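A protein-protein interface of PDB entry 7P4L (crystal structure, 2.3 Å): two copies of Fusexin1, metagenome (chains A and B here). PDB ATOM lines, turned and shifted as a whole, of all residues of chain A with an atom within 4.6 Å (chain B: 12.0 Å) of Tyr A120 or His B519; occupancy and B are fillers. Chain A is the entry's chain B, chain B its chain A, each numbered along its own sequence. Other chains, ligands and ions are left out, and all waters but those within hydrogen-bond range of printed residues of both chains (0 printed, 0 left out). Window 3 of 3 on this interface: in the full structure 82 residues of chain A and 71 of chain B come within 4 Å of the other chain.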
ATOM      1  N   ASP A  88      24.698 -29.105   5.697  1.00  0.00           N
ATOM      2  CA  ASP A  88      23.580 -29.246   6.617  1.00  0.00           C
ATOM      3  C   ASP A  88      23.183 -30.717   6.712  1.00  0.00           C
ATOM      4  O   ASP A  88      23.870 -31.603   6.195  1.00  0.00           O
ATOM      5  CB  ASP A  88      22.407 -28.369   6.167  1.00  0.00           C
ATOM      6  CG  ASP A  88      21.903 -28.726   4.774  1.00  0.00           C
ATOM      7  OD1 ASP A  88      22.339 -29.758   4.215  1.00  0.00           O
ATOM      8  OD2 ASP A  88      21.071 -27.966   4.232  1.00  0.00           O
ATOM      9  N   GLY A  89      22.075 -30.969   7.406  1.00  0.00           N
ATOM     10  CA  GLY A  89      21.499 -32.293   7.493  1.00  0.00           C
ATOM     11  C   GLY A  89      22.085 -33.188   8.561  1.00  0.00           C
ATOM     12  O   GLY A  89      21.663 -34.347   8.669  1.00  0.00           O
ATOM     13  N   SER A 118      25.529 -24.993  14.185  1.00  0.00           N
ATOM     14  CA  SER A 118      24.275 -24.430  14.654  1.00  0.00           C
ATOM     15  C   SER A 118      23.174 -25.474  14.541  1.00  0.00           C
ATOM     16  O   SER A 118      23.103 -26.207  13.551  1.00  0.00           O
ATOM     17  CB  SER A 118      23.891 -23.194  13.841  1.00  0.00           C
ATOM     18  OG  SER A 118      24.836 -22.158  14.015  1.00  0.00           O
ATOM     19  N   ARG A 119      22.308 -25.525  15.547  1.00  0.00           N
ATOM     20  CA  ARG A 119      21.127 -26.371  15.488  1.00  0.00           C
ATOM     21  C   ARG A 119      19.973 -25.615  14.838  1.00  0.00           C
ATOM     22  O   ARG A 119      19.879 -24.387  14.926  1.00  0.00           O
ATOM     23  CB  ARG A 119      20.722 -26.846  16.885  1.00  0.00           C
ATOM     24  CG  ARG A 119      20.013 -25.799  17.729  1.00  0.00           C
ATOM     25  CD  ARG A 119      19.784 -26.303  19.142  1.00  0.00           C
ATOM     26  NE  ARG A 119      19.146 -25.303  19.987  1.00  0.00           N
ATOM     27  CZ  ARG A 119      18.896 -25.468  21.279  1.00  0.00           C
ATOM     28  NH1 ARG A 119      19.222 -26.586  21.908  1.00  0.00           N
ATOM     29  NH2 ARG A 119      18.302 -24.488  21.955  1.00  0.00           N
ATOM     30  N   TYR A 120      19.117 -26.359  14.142  1.00  0.00           N
ATOM     31  CA  TYR A 120      17.893 -25.812  13.578  1.00  0.00           C
ATOM     32  C   TYR A 120      16.784 -26.849  13.683  1.00  0.00           C
ATOM     33  O   TYR A 120      17.036 -28.058  13.661  1.00  0.00           O
ATOM     34  CB  TYR A 120      18.072 -25.370  12.119  1.00  0.00           C
ATOM     35  CG  TYR A 120      18.527 -26.462  11.176  1.00  0.00           C
ATOM     36  CD1 TYR A 120      19.867 -26.821  11.086  1.00  0.00           C
ATOM     37  CD2 TYR A 120      17.619 -27.118  10.358  1.00  0.00           C
ATOM     38  CE1 TYR A 120      20.281 -27.815  10.218  1.00  0.00           C
ATOM     39  CE2 TYR A 120      18.024 -28.107   9.488  1.00  0.00           C
ATOM     40  CZ  TYR A 120      19.357 -28.452   9.419  1.00  0.00           C
ATOM     41  OH  TYR A 120      19.763 -29.443   8.554  1.00  0.00           O
ATOM     42  N   TYR A 121      15.554 -26.358  13.813  1.00  0.00           N
ATOM     43  CA  TYR A 121      14.392 -27.224  13.969  1.00  0.00           C
ATOM     44  C   TYR A 121      14.214 -28.133  12.757  1.00  0.00           C
ATOM     45  O   TYR A 121      14.278 -27.682  11.611  1.00  0.00           O
ATOM     46  CB  TYR A 121      13.142 -26.368  14.185  1.00  0.00           C
ATOM     47  CG  TYR A 121      11.895 -27.159  14.493  1.00  0.00           C
ATOM     48  CD1 TYR A 121      11.749 -27.815  15.708  1.00  0.00           C
ATOM     49  CD2 TYR A 121      10.850 -27.231  13.576  1.00  0.00           C
ATOM     50  CE1 TYR A 121      10.607 -28.537  15.994  1.00  0.00           C
ATOM     51  CE2 TYR A 121       9.704 -27.946  13.855  1.00  0.00           C
ATOM     52  CZ  TYR A 121       9.589 -28.596  15.066  1.00  0.00           C
ATOM     53  OH  TYR A 121       8.454 -29.315  15.352  1.00  0.00           O
ATOM     54  N   SER A 122      13.988 -29.421  13.018  1.00  0.00           N
ATOM     55  CA  SER A 122      13.837 -30.426  11.971  1.00  0.00           C
ATOM     56  C   SER A 122      12.599 -31.259  12.263  1.00  0.00           C
ATOM     57  O   SER A 122      12.544 -31.954  13.283  1.00  0.00           O
ATOM     58  CB  SER A 122      15.077 -31.323  11.878  1.00  0.00           C
ATOM     59  OG  SER A 122      14.928 -32.297  10.858  1.00  0.00           O
ATOM     60  N   VAL A 127      14.669 -33.420  17.673  1.00  0.00           N
ATOM     61  CA  VAL A 127      14.074 -32.085  17.592  1.00  0.00           C
ATOM     62  C   VAL A 127      14.834 -31.186  16.609  1.00  0.00           C
ATOM     63  O   VAL A 127      14.239 -30.335  15.944  1.00  0.00           O
ATOM     64  CB  VAL A 127      13.997 -31.435  18.990  1.00  0.00           C
ATOM     65  CG1 VAL A 127      13.332 -30.066  18.917  1.00  0.00           C
ATOM     66  CG2 VAL A 127      13.242 -32.338  19.950  1.00  0.00           C
ATOM     67  N   TYR A 128      16.146 -31.388  16.494  1.00  0.00           N
ATOM     68  CA  TYR A 128      16.986 -30.510  15.696  1.00  0.00           C
ATOM     69  C   TYR A 128      17.850 -31.305  14.730  1.00  0.00           C
ATOM     70  O   TYR A 128      18.189 -32.465  14.979  1.00  0.00           O
ATOM     71  CB  TYR A 128      17.911 -29.654  16.569  1.00  0.00           C
ATOM     72  CG  TYR A 128      17.220 -28.783  17.583  1.00  0.00           C
ATOM     73  CD1 TYR A 128      16.665 -27.564  17.217  1.00  0.00           C
ATOM     74  CD2 TYR A 128      17.140 -29.167  18.916  1.00  0.00           C
ATOM     75  CE1 TYR A 128      16.040 -26.754  18.149  1.00  0.00           C
ATOM     76  CE2 TYR A 128      16.515 -28.368  19.855  1.00  0.00           C
ATOM     77  CZ  TYR A 128      15.968 -27.163  19.465  1.00  0.00           C
ATOM     78  OH  TYR A 128      15.347 -26.361  20.394  1.00  0.00           O
ATOM     79  N   ASP A 129      18.200 -30.653  13.623  1.00  0.00           N
ATOM     80  CA  ASP A 129      19.348 -30.974  12.785  1.00  0.00           C
ATOM     81  C   ASP A 129      20.397 -29.876  12.949  1.00  0.00           C
ATOM     82  O   ASP A 129      20.182 -28.881  13.645  1.00  0.00           O
ATOM     83  CB  ASP A 129      18.932 -31.128  11.321  1.00  0.00           C
ATOM     84  CG  ASP A 129      18.361 -32.494  11.015  1.00  0.00           C
ATOM     85  OD1 ASP A 129      18.301 -33.334  11.937  1.00  0.00           O
ATOM     86  OD2 ASP A 129      17.979 -32.729   9.849  1.00  0.00           O
ATOM     87  N   TYR A 130      21.552 -30.061  12.310  1.00  0.00           N
ATOM     88  CA  TYR A 130      22.685 -29.178  12.554  1.00  0.00           C
ATOM     89  C   TYR A 130      23.356 -28.763  11.252  1.00  0.00           C
ATOM     90  O   TYR A 130      23.449 -29.553  10.308  1.00  0.00           O
ATOM     91  CB  TYR A 130      23.703 -29.841  13.495  1.00  0.00           C
ATOM     92  CG  TYR A 130      23.196 -29.977  14.915  1.00  0.00           C
ATOM     93  CD1 TYR A 130      22.276 -30.962  15.256  1.00  0.00           C
ATOM     94  CD2 TYR A 130      23.633 -29.114  15.913  1.00  0.00           C
ATOM     95  CE1 TYR A 130      21.799 -31.080  16.547  1.00  0.00           C
ATOM     96  CE2 TYR A 130      23.167 -29.230  17.213  1.00  0.00           C
ATOM     97  CZ  TYR A 130      22.249 -30.216  17.523  1.00  0.00           C
ATOM     98  OH  TYR A 130      21.777 -30.340  18.809  1.00  0.00           O
ATOM     99  N   GLU A 131      23.794 -27.505  11.210  1.00  0.00           N
ATOM    100  CA  GLU A 131      24.640 -26.943  10.165  1.00  0.00           C
ATOM    101  C   GLU A 131      26.054 -26.743  10.698  1.00  0.00           C
ATOM    102  O   GLU A 131      26.255 -26.553  11.900  1.00  0.00           O
ATOM    103  CB  GLU A 131      24.127 -25.581   9.695  1.00  0.00           C
ATOM    104  CG  GLU A 131      22.700 -25.506   9.324  1.00  0.00           C
ATOM    105  CD  GLU A 131      22.219 -24.074   9.248  1.00  0.00           C
ATOM    106  OE1 GLU A 131      22.190 -23.395  10.298  1.00  0.00           O
ATOM    107  OE2 GLU A 131      21.885 -23.619   8.135  1.00  0.00           O
ATOM    108  N   TYR A 133      29.834 -24.515   9.855  1.00  0.00           N
ATOM    109  CA  TYR A 133      30.508 -23.435   9.146  1.00  0.00           C
ATOM    110  C   TYR A 133      32.011 -23.638   9.280  1.00  0.00           C
ATOM    111  O   TYR A 133      32.549 -23.619  10.393  1.00  0.00           O
ATOM    112  CB  TYR A 133      30.073 -22.076   9.700  1.00  0.00           C
ATOM    113  CG  TYR A 133      28.580 -21.861   9.597  1.00  0.00           C
ATOM    114  CD1 TYR A 133      27.722 -22.333  10.582  1.00  0.00           C
ATOM    115  CD2 TYR A 133      28.028 -21.216   8.497  1.00  0.00           C
ATOM    116  CE1 TYR A 133      26.349 -22.152  10.485  1.00  0.00           C
ATOM    117  CE2 TYR A 133      26.663 -21.029   8.392  1.00  0.00           C
ATOM    118  CZ  TYR A 133      25.828 -21.500   9.390  1.00  0.00           C
ATOM    119  OH  TYR A 133      24.472 -21.328   9.291  1.00  0.00           O
ATOM    120  N   GLN A 248      28.550 -17.363  10.638  1.00  0.00           N
ATOM    121  CA  GLN A 248      27.457 -18.049  11.314  1.00  0.00           C
ATOM    122  C   GLN A 248      26.414 -17.055  11.822  1.00  0.00           C
ATOM    123  O   GLN A 248      25.210 -17.318  11.752  1.00  0.00           O
ATOM    124  CB  GLN A 248      28.024 -18.873  12.469  1.00  0.00           C
ATOM    125  CG  GLN A 248      27.012 -19.679  13.257  1.00  0.00           C
ATOM    126  CD  GLN A 248      27.670 -20.428  14.396  1.00  0.00           C
ATOM    127  OE1 GLN A 248      28.621 -19.936  14.998  1.00  0.00           O
ATOM    128  NE2 GLN A 248      27.180 -21.626  14.687  1.00  0.00           N
ATOM    129  N   GLY B 250      27.404 -15.683  25.471  1.00  0.00           N
ATOM    130  CA  GLY B 250      26.922 -17.029  25.250  1.00  0.00           C
ATOM    131  C   GLY B 250      27.516 -17.721  24.043  1.00  0.00           C
ATOM    132  O   GLY B 250      27.198 -18.891  23.800  1.00  0.00           O
ATOM    133  N   THR B 251      28.379 -17.044  23.285  1.00  0.00           N
ATOM    134  CA  THR B 251      29.043 -17.692  22.161  1.00  0.00           C
ATOM    135  C   THR B 251      29.886 -18.871  22.631  1.00  0.00           C
ATOM    136  O   THR B 251      29.938 -19.911  21.965  1.00  0.00           O
ATOM    137  CB  THR B 251      29.911 -16.678  21.417  1.00  0.00           C
ATOM    138  OG1 THR B 251      29.094 -15.592  20.957  1.00  0.00           O
ATOM    139  CG2 THR B 251      30.607 -17.334  20.230  1.00  0.00           C
ATOM    140  N   GLU B 516      22.622 -20.426   3.505  1.00  0.00           N
ATOM    141  CA  GLU B 516      23.507 -21.233   4.397  1.00  0.00           C
ATOM    142  C   GLU B 516      23.159 -21.052   5.872  1.00  0.00           C
ATOM    143  O   GLU B 516      24.010 -21.252   6.741  1.00  0.00           O
ATOM    144  CB  GLU B 516      24.974 -20.855   4.169  1.00  0.00           C
ATOM    145  CG  GLU B 516      25.535 -21.337   2.839  1.00  0.00           C
ATOM    146  CD  GLU B 516      26.244 -20.246   2.060  1.00  0.00           C
ATOM    147  OE1 GLU B 516      26.086 -19.051   2.400  1.00  0.00           O
ATOM    148  OE2 GLU B 516      26.959 -20.588   1.099  1.00  0.00           O
ATOM    149  N   HIS B 517      21.908 -20.676   6.163  1.00  0.00           N
ATOM    150  CA  HIS B 517      21.489 -20.408   7.541  1.00  0.00           C
ATOM    151  C   HIS B 517      20.062 -20.920   7.733  1.00  0.00           C
ATOM    152  O   HIS B 517      19.093 -20.182   7.531  1.00  0.00           O
ATOM    153  CB  HIS B 517      21.605 -18.922   7.859  1.00  0.00           C
ATOM    154  CG  HIS B 517      22.973 -18.359   7.622  1.00  0.00           C
ATOM    155  ND1 HIS B 517      23.452 -18.071   6.362  1.00  0.00           N
ATOM    156  CD2 HIS B 517      23.968 -18.040   8.483  1.00  0.00           C
ATOM    157  CE1 HIS B 517      24.682 -17.598   6.458  1.00  0.00           C
ATOM    158  NE2 HIS B 517      25.019 -17.568   7.734  1.00  0.00           N
ATOM    159  N   HIS B 518      19.946 -22.186   8.144  1.00  0.00           N
ATOM    160  CA  HIS B 518      18.659 -22.715   8.581  1.00  0.00           C
ATOM    161  C   HIS B 518      18.276 -22.191   9.957  1.00  0.00           C
ATOM    162  O   HIS B 518      17.091 -21.961  10.222  1.00  0.00           O
ATOM    163  CB  HIS B 518      18.686 -24.246   8.624  1.00  0.00           C
ATOM    164  CG  HIS B 518      18.940 -24.895   7.300  1.00  0.00           C
ATOM    165  ND1 HIS B 518      18.196 -24.610   6.176  1.00  0.00           N
ATOM    166  CD2 HIS B 518      19.841 -25.836   6.927  1.00  0.00           C
ATOM    167  CE1 HIS B 518      18.635 -25.337   5.164  1.00  0.00           C
ATOM    168  NE2 HIS B 518      19.634 -26.089   5.593  1.00  0.00           N
ATOM    169  N   HIS B 519      19.257 -21.981  10.839  1.00  0.00           N
ATOM    170  CA  HIS B 519      18.948 -21.481  12.172  1.00  0.00           C
ATOM    171  C   HIS B 519      18.450 -20.041  12.142  1.00  0.00           C
ATOM    172  O   HIS B 519      17.824 -19.602  13.111  1.00  0.00           O
ATOM    173  CB  HIS B 519      20.156 -21.643  13.108  1.00  0.00           C
ATOM    174  CG  HIS B 519      21.322 -20.765  12.782  1.00  0.00           C
ATOM    175  ND1 HIS B 519      22.184 -21.025  11.738  1.00  0.00           N
ATOM    176  CD2 HIS B 519      21.796 -19.654  13.393  1.00  0.00           C
ATOM    177  CE1 HIS B 519      23.123 -20.096  11.704  1.00  0.00           C
ATOM    178  NE2 HIS B 519      22.910 -19.252  12.698  1.00  0.00           N
ATOM    179  N   HIS B 520      18.737 -19.287  11.079  1.00  0.00           N
ATOM    180  CA  HIS B 520      18.192 -17.941  10.957  1.00  0.00           C
ATOM    181  C   HIS B 520      16.757 -17.937  10.444  1.00  0.00           C
ATOM    182  O   HIS B 520      16.113 -16.882  10.467  1.00  0.00           O
ATOM    183  CB  HIS B 520      19.055 -17.095  10.018  1.00  0.00           C
ATOM    184  CG  HIS B 520      20.373 -16.694  10.602  1.00  0.00           C
ATOM    185  ND1 HIS B 520      21.386 -16.148   9.845  1.00  0.00           N
ATOM    186  CD2 HIS B 520      20.840 -16.751  11.872  1.00  0.00           C
ATOM    187  CE1 HIS B 520      22.424 -15.892  10.622  1.00  0.00           C
ATOM    188  NE2 HIS B 520      22.119 -16.248  11.857  1.00  0.00           N
ATOM    189  N   HIS B 521      16.245 -19.084  10.006  1.00  0.00           N
ATOM    190  CA  HIS B 521      14.847 -19.232   9.604  1.00  0.00           C
ATOM    191  C   HIS B 521      14.385 -18.083   8.713  1.00  0.00           C
ATOM    192  O   HIS B 521      13.473 -17.337   9.069  1.00  0.00           O
ATOM    193  CB  HIS B 521      13.948 -19.329  10.840  1.00  0.00           C
ATOM    194  CG  HIS B 521      14.066 -20.632  11.571  1.00  0.00           C
ATOM    195  ND1 HIS B 521      14.704 -21.732  11.037  1.00  0.00           N
ATOM    196  CD2 HIS B 521      13.625 -21.011  12.794  1.00  0.00           C
ATOM    197  CE1 HIS B 521      14.656 -22.730  11.900  1.00  0.00           C
ATOM    198  NE2 HIS B 521      14.006 -22.320  12.975  1.00  0.00           N
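The backbone carbonyl oxygen (O) of Glu B516 lies within hydrogen-bond range of the side-chain hydroxyl (OH) of Tyr A133 (2.6 Å). A ring nitrogen (NE2) of His B518 is in hydrogen-bond range of the side-chain carboxylate of Asp A88, at 2.7 Å. The side-chain carboxylate of Glu A131 is in hydrogen-bond range of the backbone NH of His B518. A ring nitrogen (ND1) of His B519 is in hydrogen-bond range of the side-chain carboxylate (OE1) of Glu A131, 2.8 Å away. ND1 of His B519 lies close to OH of Tyr A133. A ring nitrogen (NE2) of His B519 sits at hydrogen-bond distance from the backbone carbonyl oxygen of Gln A248 (3.2 Å). NE2 of His B520 is in hydrogen-bond range of O of Gln A248, 3.3 Å away. The side-chain carboxylate (OE2) of Glu A131 lies close to the backbone carbonyl oxygen (O) of Glu B516 (3.5 Å).
A ring nitrogen (ND1) of His B521 lies within hydrogen-bond range of the backbone carbonyl oxygen of His B518, 2.5 Å away. NE2 of His B519 sits at hydrogen-bond distance from NE2 of His B520. The backbone carbonyl oxygen (O) of Ser A118 lies within hydrogen-bond range of the backbone NH (N) of Glu A131 (2.8 Å). The side-chain hydroxyl (OG) of Ser A118 lies within hydrogen-bond range of the side-chain amide nitrogen (NE2) of Gln A248, at 2.5 Å. The backbone NH (N) of Tyr A120 lies within hydrogen-bond range of the backbone carbonyl oxygen (O) of Asp A129. The side-chain hydroxyl (OH) of Tyr A133 lies within hydrogen-bond range of the side-chain carboxylate (OE1) of Glu A131.
Among the printed residues, merely in contact across the chains: Glu A131 with His B517 (3.3 Å), Arg A119 with His B519 (3.3 Å), Tyr A120 with His B518 (3.4 Å), Tyr A133 with His B517 (3.4 Å), Ser A118 with His B519 (3.5 Å), Gln A248 with His B517 (3.6 Å) and Tyr A120 with His B519 (3.8 Å).
Of chain B, only His B518 (2.7 Å) comes within 4 Å of Asp A88. No residue of chain B comes within 4 Å of Gly A89. Of chain B, only His B519 comes within 4 Å of Ser A118. Tyr A120 touches two residues of chain B. No residue of chain B comes within 4 Å of Ser A122. Val A127 touches none of the printed residues of chain B. No residue of chain B comes within 4 Å of Tyr A128. No residue of chain B comes within 4 Å of Tyr A130. Glu A131 touches just these residues of chain B: Glu B516 (3.5 Å), His B517 (3.3 Å), His B518 (2.4 Å) and His B519 (2.8 Å). Printed residues of chain B within 4 Å of Tyr A133: Glu B516 (2.6 Å), His B517 (3.4 Å) and His B519 (3.0 Å). Gln A248 touches just these residues of chain B: His B517 (3.6 Å), His B519 (3.2 Å) and His B520 (3.3 Å). Of the printed residues of chain A, His B517 touches Glu A131, Tyr A133 and Gln A248. Of the printed residues of chain A, His B518 touches Asp A88, Tyr A120 and Glu A131. Printed residues of chain A within 4 Å of His B519: Ser A118 (3.5 Å), Arg A119 (3.3 Å), Tyr A120 (3.8 Å), Glu A131 (2.8 Å), Tyr A133 (3.0 Å) and Gln A248 (3.2 Å). Printed residues of chain A within 4 Å of His B520: Gln A248.
Of the 8 printed residues of chain B, 5 touch a printed residue of chain A. Hydrophobic or aromatic side chains of chain B within 4 Å of the printed part of chain A: His B517, His B518, His B519 and His B520. Printed residues of chain A that touch a printed residue of chain B: Asp A88, Ser A118, Arg A119, Tyr A120, Glu A131, Tyr A133 and Gln A248. Hydrophobic or aromatic side chains of chain A that line the printed part of chain B: Tyr A120 and Tyr A133. Among the printed residues, 15 pairs touch across the chains.
No position is printed for both chains. Of the 15 pairs that touch across the chains among the printed residues, none has its exchanged pair printed and touching as well.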
